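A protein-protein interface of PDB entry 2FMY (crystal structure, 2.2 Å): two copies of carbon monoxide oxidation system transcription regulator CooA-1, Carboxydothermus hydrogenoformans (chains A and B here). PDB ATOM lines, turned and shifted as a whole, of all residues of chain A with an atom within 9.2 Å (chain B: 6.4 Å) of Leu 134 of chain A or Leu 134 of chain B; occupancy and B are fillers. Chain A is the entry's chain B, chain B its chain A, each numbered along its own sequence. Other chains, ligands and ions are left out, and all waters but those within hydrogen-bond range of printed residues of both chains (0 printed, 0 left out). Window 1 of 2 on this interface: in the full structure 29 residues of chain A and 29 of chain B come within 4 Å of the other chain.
The side-chain hydroxyl (OH) of Tyr 62 of chain A lies within hydrogen-bond range of the side-chain amide oxygen (OD1) of Asn 132 of chain B (2.7 Å).
Ile 131 of chain B touches Leu 60 of chain A (CG2 to CD1, 3.7 Å).
CG2 of Ile 131 of chain B touches OH of Tyr 62 of chain A, at 3.5 Å.
CG1 of Val 135 of chain B touches CD2 of Tyr 62 of chain A, 3.99 Å away.
Phe 136 of chain B touches Tyr 62 of chain A.
Lys 65 of chain A touches Val 135 of chain B.
Ser 127 of chain A touches Ile 131 of chain B.
Ile 131 of chain A touches Ile 131 of chain B.
Leu 134 of chain A touches Leu 134 of chain B.
Leu 134 of chain A touches Val 135 of chain B (CD1 to CG2, 3.98 Å).
CG2 of Val 135 of chain A touches CE1 of Phe 67 of chain B (3.96 Å).
The backbone NH (N) of Phe 67 of chain A is in hydrogen-bond range of the backbone carbonyl oxygen (O) of Leu 60 of chain A, at 2.8 Å.
Of the printed residues of chain B, Leu 60 of chain A touches Ile 131.
Of the printed residues of chain B, Tyr 62 of chain A touches Ile 131 (3.5 Å), Asn 132 (2.7 Å), Val 135 (3.99 Å) and Phe 136 (3.5 Å).
Asp 138 of chain A touches none of the printed residues of chain B.
Of the printed residues of chain A, Ile 130 of chain B touches Ile 131.
Of the printed residues of chain A, Ile 131 of chain B touches Leu 60, Tyr 62, Ser 127, Ile 130 and Ile 131.
No residue of chain A comes within 4 Å of Gly 133 of chain B.
Leu 134 of chain B touches just one residue of chain A: Leu 134 (3.9 Å).
The nearest residue of chain A that does not touch Leu 134 of chain B is Ile 131 of chain A (4.04 Å).
Hydrophobic or aromatic side chains of chain B that line the printed part of chain A: Phe 67, Ile 130, Ile 131, Leu 134, Val 135 and Phe 136.
Hydrophobic or aromatic side chains of chain A within 4 Å of the printed part of chain B: Leu 60, Tyr 62, Phe 67, Ile 130, Ile 131, Leu 134 and Val 135.
Phe 67 of chain A touches Val 135 of chain B, and with the chains exchanged Val 135 of chain A touches Phe 67 of chain B.
Ile 130 of chain A touches Ile 131 of chain B, and with the chains exchanged Ile 131 of chain A touches Ile 130 of chain B.
Ile 131 of chain A touches its own counterpart, Ile 131 of chain B.
Leu 134 of chain A touches Val 135 of chain B, but with the chains exchanged Val 135 of chain A does not touch Leu 134 of chain B (4.3 Å).
Of the 14 pairs that touch across the chains among the printed residues, 6 have their exchanged pair printed and touching as well.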
ATOM      1  N   LEU A  60     -10.576   8.700  22.654  1.00  0.00           N
ATOM      2  CA  LEU A  60      -9.521   8.710  21.655  1.00  0.00           C
ATOM      3  C   LEU A  60      -9.517  10.080  21.008  1.00  0.00           C
ATOM      4  O   LEU A  60     -10.566  10.570  20.576  1.00  0.00           O
ATOM      5  CB  LEU A  60      -9.784   7.648  20.590  1.00  0.00           C
ATOM      6  CG  LEU A  60      -9.776   6.174  21.007  1.00  0.00           C
ATOM      7  CD1 LEU A  60     -10.449   5.314  19.949  1.00  0.00           C
ATOM      8  CD2 LEU A  60      -8.368   5.683  21.293  1.00  0.00           C
ATOM      9  N   TYR A  62      -7.885  12.561  18.020  1.00  0.00           N
ATOM     10  CA  TYR A  62      -7.167  12.740  16.763  1.00  0.00           C
ATOM     11  C   TYR A  62      -7.086  14.234  16.478  1.00  0.00           C
ATOM     12  O   TYR A  62      -7.499  15.038  17.312  1.00  0.00           O
ATOM     13  CB  TYR A  62      -7.881  11.991  15.637  1.00  0.00           C
ATOM     14  CG  TYR A  62      -8.093  10.527  15.953  1.00  0.00           C
ATOM     15  CD1 TYR A  62      -9.332  10.069  16.413  1.00  0.00           C
ATOM     16  CD2 TYR A  62      -7.055   9.606  15.822  1.00  0.00           C
ATOM     17  CE1 TYR A  62      -9.532   8.741  16.717  1.00  0.00           C
ATOM     18  CE2 TYR A  62      -7.249   8.259  16.130  1.00  0.00           C
ATOM     19  CZ  TYR A  62      -8.491   7.837  16.576  1.00  0.00           C
ATOM     20  OH  TYR A  62      -8.707   6.514  16.874  1.00  0.00           O
ATOM     21  N   LYS A  65     -11.016  15.108  15.229  1.00  0.00           N
ATOM     22  CA  LYS A  65     -12.137  14.488  15.935  1.00  0.00           C
ATOM     23  C   LYS A  65     -11.704  13.757  17.203  1.00  0.00           C
ATOM     24  O   LYS A  65     -10.542  13.374  17.354  1.00  0.00           O
ATOM     25  CB  LYS A  65     -12.899  13.522  15.011  1.00  0.00           C
ATOM     26  CG  LYS A  65     -12.049  12.408  14.398  1.00  0.00           C
ATOM     27  CD  LYS A  65     -12.822  11.665  13.315  1.00  0.00           C
ATOM     28  CE  LYS A  65     -11.933  10.695  12.542  1.00  0.00           C
ATOM     29  NZ  LYS A  65     -10.908  11.421  11.724  1.00  0.00           N
ATOM     30  N   PHE A  67     -13.314  10.574  19.879  1.00  0.00           N
ATOM     31  CA  PHE A  67     -14.334   9.573  20.139  1.00  0.00           C
ATOM     32  C   PHE A  67     -14.396   9.271  21.618  1.00  0.00           C
ATOM     33  O   PHE A  67     -13.421   8.815  22.205  1.00  0.00           O
ATOM     34  CB  PHE A  67     -14.056   8.287  19.364  1.00  0.00           C
ATOM     35  CG  PHE A  67     -14.134   8.445  17.878  1.00  0.00           C
ATOM     36  CD1 PHE A  67     -13.020   8.208  17.091  1.00  0.00           C
ATOM     37  CD2 PHE A  67     -15.320   8.844  17.263  1.00  0.00           C
ATOM     38  CE1 PHE A  67     -13.080   8.361  15.704  1.00  0.00           C
ATOM     39  CE2 PHE A  67     -15.388   9.002  15.878  1.00  0.00           C
ATOM     40  CZ  PHE A  67     -14.261   8.756  15.101  1.00  0.00           C
ATOM     41  N   ASN A 126     -19.206   1.221  23.556  1.00  0.00           N
ATOM     42  CA  ASN A 126     -18.988   2.440  22.797  1.00  0.00           C
ATOM     43  C   ASN A 126     -18.022   2.262  21.634  1.00  0.00           C
ATOM     44  O   ASN A 126     -18.194   2.906  20.599  1.00  0.00           O
ATOM     45  CB  ASN A 126     -18.547   3.569  23.725  1.00  0.00           C
ATOM     46  CG  ASN A 126     -19.603   3.884  24.782  1.00  0.00           C
ATOM     47  OD1 ASN A 126     -20.754   4.121  24.451  1.00  0.00           O
ATOM     48  ND2 ASN A 126     -19.220   3.855  26.050  1.00  0.00           N
ATOM     49  N   SER A 127     -17.034   1.374  21.808  1.00  0.00           N
ATOM     50  CA  SER A 127     -16.061   1.029  20.767  1.00  0.00           C
ATOM     51  C   SER A 127     -16.721   0.391  19.540  1.00  0.00           C
ATOM     52  O   SER A 127     -16.410   0.765  18.416  1.00  0.00           O
ATOM     53  CB  SER A 127     -14.976   0.083  21.309  1.00  0.00           C
ATOM     54  OG  SER A 127     -14.146   0.742  22.255  1.00  0.00           O
ATOM     55  N   LEU A 128     -17.600  -0.587  19.774  1.00  0.00           N
ATOM     56  CA  LEU A 128     -18.375  -1.232  18.716  1.00  0.00           C
ATOM     57  C   LEU A 128     -19.248  -0.238  17.948  1.00  0.00           C
ATOM     58  O   LEU A 128     -19.332  -0.304  16.730  1.00  0.00           O
ATOM     59  CB  LEU A 128     -19.222  -2.387  19.271  1.00  0.00           C
ATOM     60  CG  LEU A 128     -18.484  -3.484  20.040  1.00  0.00           C
ATOM     61  CD1 LEU A 128     -19.414  -4.666  20.368  1.00  0.00           C
ATOM     62  CD2 LEU A 128     -17.209  -3.944  19.317  1.00  0.00           C
ATOM     63  N   THR A 129     -19.873   0.688  18.664  1.00  0.00           N
ATOM     64  CA  THR A 129     -20.638   1.770  18.045  1.00  0.00           C
ATOM     65  C   THR A 129     -19.755   2.623  17.124  1.00  0.00           C
ATOM     66  O   THR A 129     -20.147   2.932  15.986  1.00  0.00           O
ATOM     67  CB  THR A 129     -21.342   2.629  19.118  1.00  0.00           C
ATOM     68  OG1 THR A 129     -22.295   1.810  19.807  1.00  0.00           O
ATOM     69  CG2 THR A 129     -22.065   3.821  18.498  1.00  0.00           C
ATOM     70  N   ILE A 130     -18.567   2.972  17.620  1.00  0.00           N
ATOM     71  CA  ILE A 130     -17.561   3.748  16.872  1.00  0.00           C
ATOM     72  C   ILE A 130     -17.097   3.032  15.591  1.00  0.00           C
ATOM     73  O   ILE A 130     -16.960   3.652  14.532  1.00  0.00           O
ATOM     74  CB  ILE A 130     -16.337   4.099  17.773  1.00  0.00           C
ATOM     75  CG1 ILE A 130     -16.740   5.157  18.816  1.00  0.00           C
ATOM     76  CG2 ILE A 130     -15.166   4.622  16.932  1.00  0.00           C
ATOM     77  CD1 ILE A 130     -15.839   5.179  20.047  1.00  0.00           C
ATOM     78  N   ILE A 131     -16.867   1.729  15.696  1.00  0.00           N
ATOM     79  CA  ILE A 131     -16.451   0.912  14.557  1.00  0.00           C
ATOM     80  C   ILE A 131     -17.562   0.835  13.500  1.00  0.00           C
ATOM     81  O   ILE A 131     -17.305   1.029  12.312  1.00  0.00           O
ATOM     82  CB  ILE A 131     -15.979  -0.502  15.003  1.00  0.00           C
ATOM     83  CG1 ILE A 131     -14.656  -0.404  15.770  1.00  0.00           C
ATOM     84  CG2 ILE A 131     -15.781  -1.412  13.800  1.00  0.00           C
ATOM     85  CD1 ILE A 131     -14.396  -1.542  16.726  1.00  0.00           C
ATOM     86  N   ASN A 132     -18.792   0.553  13.938  1.00  0.00           N
ATOM     87  CA  ASN A 132     -19.975   0.623  13.072  1.00  0.00           C
ATOM     88  C   ASN A 132     -20.107   2.007  12.396  1.00  0.00           C
ATOM     89  O   ASN A 132     -20.413   2.095  11.203  1.00  0.00           O
ATOM     90  CB  ASN A 132     -21.243   0.310  13.874  1.00  0.00           C
ATOM     91  CG  ASN A 132     -21.546  -1.187  13.976  1.00  0.00           C
ATOM     92  OD1 ASN A 132     -20.913  -2.014  13.336  1.00  0.00           O
ATOM     93  ND2 ASN A 132     -22.537  -1.529  14.789  1.00  0.00           N
ATOM     94  N   GLY A 133     -19.878   3.067  13.171  1.00  0.00           N
ATOM     95  CA  GLY A 133     -19.936   4.449  12.690  1.00  0.00           C
ATOM     96  C   GLY A 133     -18.856   4.815  11.686  1.00  0.00           C
ATOM     97  O   GLY A 133     -19.076   5.647  10.820  1.00  0.00           O
ATOM     98  N   LEU A 134     -17.688   4.190  11.797  1.00  0.00           N
ATOM     99  CA  LEU A 134     -16.624   4.372  10.811  1.00  0.00           C
ATOM    100  C   LEU A 134     -16.839   3.549   9.537  1.00  0.00           C
ATOM    101  O   LEU A 134     -16.669   4.068   8.433  1.00  0.00           O
ATOM    102  CB  LEU A 134     -15.250   4.078  11.434  1.00  0.00           C
ATOM    103  CG  LEU A 134     -14.767   5.170  12.401  1.00  0.00           C
ATOM    104  CD1 LEU A 134     -13.720   4.626  13.338  1.00  0.00           C
ATOM    105  CD2 LEU A 134     -14.240   6.390  11.655  1.00  0.00           C
ATOM    106  N   VAL A 135     -17.223   2.281   9.687  1.00  0.00           N
ATOM    107  CA  VAL A 135     -17.568   1.455   8.527  1.00  0.00           C
ATOM    108  C   VAL A 135     -18.716   2.071   7.707  1.00  0.00           C
ATOM    109  O   VAL A 135     -18.661   2.064   6.475  1.00  0.00           O
ATOM    110  CB  VAL A 135     -17.884  -0.007   8.914  1.00  0.00           C
ATOM    111  CG1 VAL A 135     -18.460  -0.773   7.727  1.00  0.00           C
ATOM    112  CG2 VAL A 135     -16.627  -0.715   9.417  1.00  0.00           C
ATOM    113  N   PHE A 136     -19.735   2.605   8.394  1.00  0.00           N
ATOM    114  CA  PHE A 136     -20.901   3.236   7.760  1.00  0.00           C
ATOM    115  C   PHE A 136     -20.912   4.763   7.945  1.00  0.00           C
ATOM    116  O   PHE A 136     -21.970   5.350   8.149  1.00  0.00           O
ATOM    117  CB  PHE A 136     -22.212   2.674   8.335  1.00  0.00           C
ATOM    118  CG  PHE A 136     -22.372   1.184   8.194  1.00  0.00           C
ATOM    119  CD1 PHE A 136     -22.518   0.386   9.325  1.00  0.00           C
ATOM    120  CD2 PHE A 136     -22.405   0.578   6.935  1.00  0.00           C
ATOM    121  CE1 PHE A 136     -22.681  -0.992   9.214  1.00  0.00           C
ATOM    122  CE2 PHE A 136     -22.564  -0.806   6.812  1.00  0.00           C
ATOM    123  CZ  PHE A 136     -22.708  -1.589   7.956  1.00  0.00           C
ATOM    124  N   LYS A 137     -19.745   5.402   7.871  1.00  0.00           N
ATOM    125  CA  LYS A 137     -19.633   6.840   8.151  1.00  0.00           C
ATOM    126  C   LYS A 137     -20.685   7.686   7.416  1.00  0.00           C
ATOM    127  O   LYS A 137     -21.405   8.452   8.045  1.00  0.00           O
ATOM    128  CB  LYS A 137     -18.216   7.347   7.892  1.00  0.00           C
ATOM    129  CG  LYS A 137     -17.908   8.727   8.487  1.00  0.00           C
ATOM    130  CD  LYS A 137     -16.429   9.066   8.336  1.00  0.00           C
ATOM    131  CE  LYS A 137     -16.149  10.541   8.596  1.00  0.00           C
ATOM    132  NZ  LYS A 137     -14.676  10.871   8.508  1.00  0.00           N
ATOM    133  N   ASP A 138     -20.790   7.506   6.102  1.00  0.00           N
ATOM    134  CA  ASP A 138     -21.653   8.340   5.264  1.00  0.00           C
ATOM    135  C   ASP A 138     -23.142   8.064   5.462  1.00  0.00           C
ATOM    136  O   ASP A 138     -23.921   8.993   5.651  1.00  0.00           O
ATOM    137  CB  ASP A 138     -21.244   8.229   3.788  1.00  0.00           C
ATOM    138  CG  ASP A 138     -19.878   8.822   3.528  1.00  0.00           C
ATOM    139  OD1 ASP A 138     -19.449   8.865   2.357  1.00  0.00           O
ATOM    140  OD2 ASP A 138     -19.221   9.257   4.498  1.00  0.00           O
ATOM    141  N   ALA A 139     -23.526   6.790   5.425  1.00  0.00           N
ATOM    142  CA  ALA A 139     -24.876   6.375   5.764  1.00  0.00           C
ATOM    143  C   ALA A 139     -25.292   6.876   7.148  1.00  0.00           C
ATOM    144  O   ALA A 139     -26.420   7.310   7.337  1.00  0.00           O
ATOM    145  CB  ALA A 139     -24.995   4.859   5.699  1.00  0.00           C
ATOM    146  N   ARG A 140     -24.383   6.804   8.117  1.00  0.00           N
ATOM    147  CA  ARG A 140     -24.682   7.262   9.474  1.00  0.00           C
ATOM    148  C   ARG A 140     -24.976   8.758   9.508  1.00  0.00           C
ATOM    149  O   ARG A 140     -25.957   9.184  10.118  1.00  0.00           O
ATOM    150  CB  ARG A 140     -23.525   6.949  10.405  1.00  0.00           C
ATOM    151  CG  ARG A 140     -23.849   7.122  11.863  1.00  0.00           C
ATOM    152  CD  ARG A 140     -22.564   7.351  12.624  1.00  0.00           C
ATOM    153  NE  ARG A 140     -22.672   6.833  13.971  1.00  0.00           N
ATOM    154  CZ  ARG A 140     -21.746   6.974  14.913  1.00  0.00           C
ATOM    155  NH1 ARG A 140     -20.631   7.649  14.671  1.00  0.00           N
ATOM    156  NH2 ARG A 140     -21.959   6.450  16.110  1.00  0.00           N
ATOM    157  N   LEU A 141     -24.116   9.543   8.867  1.00  0.00           N
ATOM    158  CA  LEU A 141     -24.317  10.984   8.758  1.00  0.00           C
ATOM    159  C   LEU A 141     -25.677  11.311   8.130  1.00  0.00           C
ATOM    160  O   LEU A 141     -26.437  12.090   8.685  1.00  0.00           O
ATOM    161  CB  LEU A 141     -23.170  11.629   7.969  1.00  0.00           C
ATOM    162  CG  LEU A 141     -23.121  13.155   7.836  1.00  0.00           C
ATOM    163  CD1 LEU A 141     -23.123  13.815   9.206  1.00  0.00           C
ATOM    164  CD2 LEU A 141     -21.890  13.587   7.046  1.00  0.00           C
ATOM    165  N   LEU A 187     -27.554   0.804  12.239  1.00  0.00           N
ATOM    166  CA  LEU A 187     -27.368   2.165  12.754  1.00  0.00           C
ATOM    167  C   LEU A 187     -28.452   2.607  13.750  1.00  0.00           C
ATOM    168  O   LEU A 187     -28.154   3.280  14.740  1.00  0.00           O
ATOM    169  CB  LEU A 187     -27.215   3.165  11.594  1.00  0.00           C
ATOM    170  CG  LEU A 187     -25.965   3.002  10.700  1.00  0.00           C
ATOM    171  CD1 LEU A 187     -26.075   3.804   9.419  1.00  0.00           C
ATOM    172  CD2 LEU A 187     -24.665   3.364  11.433  1.00  0.00           C
ATOM    173  N   ASP A 190     -27.849   0.868  16.998  1.00  0.00           N
ATOM    174  CA  ASP A 190     -26.738   1.561  17.660  1.00  0.00           C
ATOM    175  C   ASP A 190     -27.208   2.824  18.371  1.00  0.00           C
ATOM    176  O   ASP A 190     -26.780   3.092  19.488  1.00  0.00           O
ATOM    177  CB  ASP A 190     -25.646   1.926  16.651  1.00  0.00           C
ATOM    178  CG  ASP A 190     -24.752   0.753  16.297  1.00  0.00           C
ATOM    179  OD1 ASP A 190     -24.919  -0.334  16.889  1.00  0.00           O
ATOM    180  OD2 ASP A 190     -23.871   0.934  15.424  1.00  0.00           O
ATOM    181  N   PHE A 216     -23.988  13.778  15.812  1.00  0.00           N
ATOM    182  CA  PHE A 216     -23.749  12.786  14.752  1.00  0.00           C
ATOM    183  C   PHE A 216     -24.199  13.255  13.367  1.00  0.00           C
ATOM    184  O   PHE A 216     -23.941  12.580  12.365  1.00  0.00           O
ATOM    185  CB  PHE A 216     -24.416  11.451  15.099  1.00  0.00           C
ATOM    186  CG  PHE A 216     -23.919  10.849  16.373  1.00  0.00           C
ATOM    187  CD1 PHE A 216     -22.793  10.035  16.377  1.00  0.00           C
ATOM    188  CD2 PHE A 216     -24.561  11.113  17.578  1.00  0.00           C
ATOM    189  CE1 PHE A 216     -22.319   9.481  17.562  1.00  0.00           C
ATOM    190  CE2 PHE A 216     -24.095  10.571  18.769  1.00  0.00           C
ATOM    191  CZ  PHE A 216     -22.968   9.755  18.759  1.00  0.00           C
ATOM    192  N   PHE B  67     -14.144  -8.149  11.128  1.00  0.00           N
ATOM    193  CA  PHE B  67     -13.126  -7.739  12.081  1.00  0.00           C
ATOM    194  C   PHE B  67     -13.153  -8.690  13.274  1.00  0.00           C
ATOM    195  O   PHE B  67     -14.113  -8.699  14.052  1.00  0.00           O
ATOM    196  CB  PHE B  67     -13.368  -6.295  12.566  1.00  0.00           C
ATOM    197  CG  PHE B  67     -13.102  -5.241  11.527  1.00  0.00           C
ATOM    198  CD1 PHE B  67     -14.149  -4.530  10.957  1.00  0.00           C
ATOM    199  CD2 PHE B  67     -11.798  -4.951  11.123  1.00  0.00           C
ATOM    200  CE1 PHE B  67     -13.910  -3.543   9.998  1.00  0.00           C
ATOM    201  CE2 PHE B  67     -11.547  -3.971  10.161  1.00  0.00           C
ATOM    202  CZ  PHE B  67     -12.609  -3.267   9.595  1.00  0.00           C
ATOM    203  N   THR B 129      -7.336  -0.871  18.352  1.00  0.00           N
ATOM    204  CA  THR B 129      -6.489  -1.081  17.183  1.00  0.00           C
ATOM    205  C   THR B 129      -7.305  -0.998  15.881  1.00  0.00           C
ATOM    206  O   THR B 129      -6.862  -0.400  14.904  1.00  0.00           O
ATOM    207  CB  THR B 129      -5.720  -2.421  17.319  1.00  0.00           C
ATOM    208  OG1 THR B 129      -4.851  -2.332  18.455  1.00  0.00           O
ATOM    209  CG2 THR B 129      -4.874  -2.727  16.071  1.00  0.00           C
ATOM    210  N   ILE B 130      -8.496  -1.596  15.878  1.00  0.00           N
ATOM    211  CA  ILE B 130      -9.396  -1.538  14.715  1.00  0.00           C
ATOM    212  C   ILE B 130      -9.818  -0.093  14.410  1.00  0.00           C
ATOM    213  O   ILE B 130      -9.771   0.341  13.258  1.00  0.00           O
ATOM    214  CB  ILE B 130     -10.636  -2.478  14.896  1.00  0.00           C
ATOM    215  CG1 ILE B 130     -10.186  -3.943  14.823  1.00  0.00           C
ATOM    216  CG2 ILE B 130     -11.720  -2.193  13.838  1.00  0.00           C
ATOM    217  CD1 ILE B 130     -11.149  -4.923  15.466  1.00  0.00           C
ATOM    218  N   ILE B 131     -10.203   0.642  15.450  1.00  0.00           N
ATOM    219  CA  ILE B 131     -10.590   2.045  15.324  1.00  0.00           C
ATOM    220  C   ILE B 131      -9.474   2.877  14.702  1.00  0.00           C
ATOM    221  O   ILE B 131      -9.692   3.567  13.693  1.00  0.00           O
ATOM    222  CB  ILE B 131     -11.061   2.635  16.678  1.00  0.00           C
ATOM    223  CG1 ILE B 131     -12.364   1.957  17.117  1.00  0.00           C
ATOM    224  CG2 ILE B 131     -11.271   4.160  16.572  1.00  0.00           C
ATOM    225  CD1 ILE B 131     -12.764   2.247  18.555  1.00  0.00           C
ATOM    226  N   ASN B 132      -8.271   2.782  15.278  1.00  0.00           N
ATOM    227  CA  ASN B 132      -7.098   3.452  14.726  1.00  0.00           C
ATOM    228  C   ASN B 132      -6.835   3.029  13.283  1.00  0.00           C
ATOM    229  O   ASN B 132      -6.486   3.854  12.437  1.00  0.00           O
ATOM    230  CB  ASN B 132      -5.859   3.181  15.590  1.00  0.00           C
ATOM    231  CG  ASN B 132      -5.826   4.016  16.861  1.00  0.00           C
ATOM    232  OD1 ASN B 132      -6.493   5.045  16.970  1.00  0.00           O
ATOM    233  ND2 ASN B 132      -5.044   3.569  17.830  1.00  0.00           N
ATOM    234  N   GLY B 133      -7.016   1.738  13.009  1.00  0.00           N
ATOM    235  CA  GLY B 133      -6.856   1.198  11.660  1.00  0.00           C
ATOM    236  C   GLY B 133      -7.837   1.786  10.649  1.00  0.00           C
ATOM    237  O   GLY B 133      -7.488   1.955   9.492  1.00  0.00           O
ATOM    238  N   LEU B 134      -9.067   2.077  11.086  1.00  0.00           N
ATOM    239  CA  LEU B 134     -10.093   2.664  10.204  1.00  0.00           C
ATOM    240  C   LEU B 134      -9.879   4.158   9.975  1.00  0.00           C
ATOM    241  O   LEU B 134      -9.993   4.638   8.848  1.00  0.00           O
ATOM    242  CB  LEU B 134     -11.503   2.410  10.754  1.00  0.00           C
ATOM    243  CG  LEU B 134     -12.093   1.006  10.577  1.00  0.00           C
ATOM    244  CD1 LEU B 134     -13.177   0.749  11.592  1.00  0.00           C
ATOM    245  CD2 LEU B 134     -12.621   0.790   9.157  1.00  0.00           C
ATOM    246  N   VAL B 135      -9.586   4.886  11.053  1.00  0.00           N
ATOM    247  CA  VAL B 135      -9.279   6.316  10.991  1.00  0.00           C
ATOM    248  C   VAL B 135      -8.067   6.628  10.089  1.00  0.00           C
ATOM    249  O   VAL B 135      -8.077   7.612   9.347  1.00  0.00           O
ATOM    250  CB  VAL B 135      -9.087   6.898  12.413  1.00  0.00           C
ATOM    251  CG1 VAL B 135      -8.573   8.328  12.364  1.00  0.00           C
ATOM    252  CG2 VAL B 135     -10.402   6.821  13.197  1.00  0.00           C
ATOM    253  N   PHE B 136      -7.043   5.774  10.145  1.00  0.00           N
ATOM    254  CA  PHE B 136      -5.819   5.963   9.371  1.00  0.00           C
ATOM    255  C   PHE B 136      -5.585   4.865   8.344  1.00  0.00           C
ATOM    256  O   PHE B 136      -4.441   4.460   8.143  1.00  0.00           O
ATOM    257  CB  PHE B 136      -4.597   6.007  10.294  1.00  0.00           C
ATOM    258  CG  PHE B 136      -4.635   7.095  11.329  1.00  0.00           C
ATOM    259  CD1 PHE B 136      -4.457   6.788  12.673  1.00  0.00           C
ATOM    260  CD2 PHE B 136      -4.826   8.424  10.965  1.00  0.00           C
ATOM    261  CE1 PHE B 136      -4.473   7.786  13.637  1.00  0.00           C
ATOM    262  CE2 PHE B 136      -4.843   9.424  11.922  1.00  0.00           C
ATOM    263  CZ  PHE B 136      -4.669   9.100  13.265  1.00  0.00           C
ATOM    264  N   LYS B 137      -6.641   4.405   7.676  1.00  0.00           N
ATOM    265  CA  LYS B 137      -6.524   3.262   6.759  1.00  0.00           C
ATOM    266  C   LYS B 137      -5.418   3.397   5.702  1.00  0.00           C
ATOM    267  O   LYS B 137      -4.626   2.468   5.518  1.00  0.00           O
ATOM    268  CB  LYS B 137      -7.861   2.934   6.094  1.00  0.00           C
ATOM    269  CG  LYS B 137      -7.896   1.558   5.418  1.00  0.00           C
ATOM    270  CD  LYS B 137      -9.220   1.307   4.705  1.00  0.00           C
ATOM    271  CE  LYS B 137     -10.316   0.848   5.672  1.00  0.00           C
ATOM    272  NZ  LYS B 137     -10.336  -0.632   5.905  1.00  0.00           N
ATOM    273  N   ASP B 138      -5.369   4.548   5.032  1.00  0.00           N
ATOM    274  CA  ASP B 138      -4.392   4.809   3.972  1.00  0.00           C
ATOM    275  C   ASP B 138      -2.971   4.885   4.509  1.00  0.00           C
ATOM    276  O   ASP B 138      -2.077   4.190   4.025  1.00  0.00           O
ATOM    277  CB  ASP B 138      -4.736   6.107   3.229  1.00  0.00           C
ATOM    278  CG  ASP B 138      -6.015   6.003   2.415  1.00  0.00           C
ATOM    279  OD1 ASP B 138      -6.465   7.046   1.889  1.00  0.00           O
ATOM    280  OD2 ASP B 138      -6.576   4.888   2.293  1.00  0.00           O
ATOM    281  N   ARG B 140      -1.816   3.788   7.325  1.00  0.00           N
ATOM    282  CA  ARG B 140      -1.432   2.487   7.874  1.00  0.00           C
ATOM    283  C   ARG B 140      -0.855   1.563   6.800  1.00  0.00           C
ATOM    284  O   ARG B 140       0.202   0.955   6.993  1.00  0.00           O
ATOM    285  CB  ARG B 140      -2.643   1.832   8.531  1.00  0.00           C
ATOM    286  CG  ARG B 140      -2.347   0.640   9.415  1.00  0.00           C
ATOM    287  CD  ARG B 140      -3.607  -0.208   9.477  1.00  0.00           C
ATOM    288  NE  ARG B 140      -3.724  -0.942  10.721  1.00  0.00           N
ATOM    289  CZ  ARG B 140      -4.730  -1.758  11.029  1.00  0.00           C
ATOM    290  NH1 ARG B 140      -5.713  -1.981  10.173  1.00  0.00           N
ATOM    291  NH2 ARG B 140      -4.735  -2.368  12.199  1.00  0.00           N
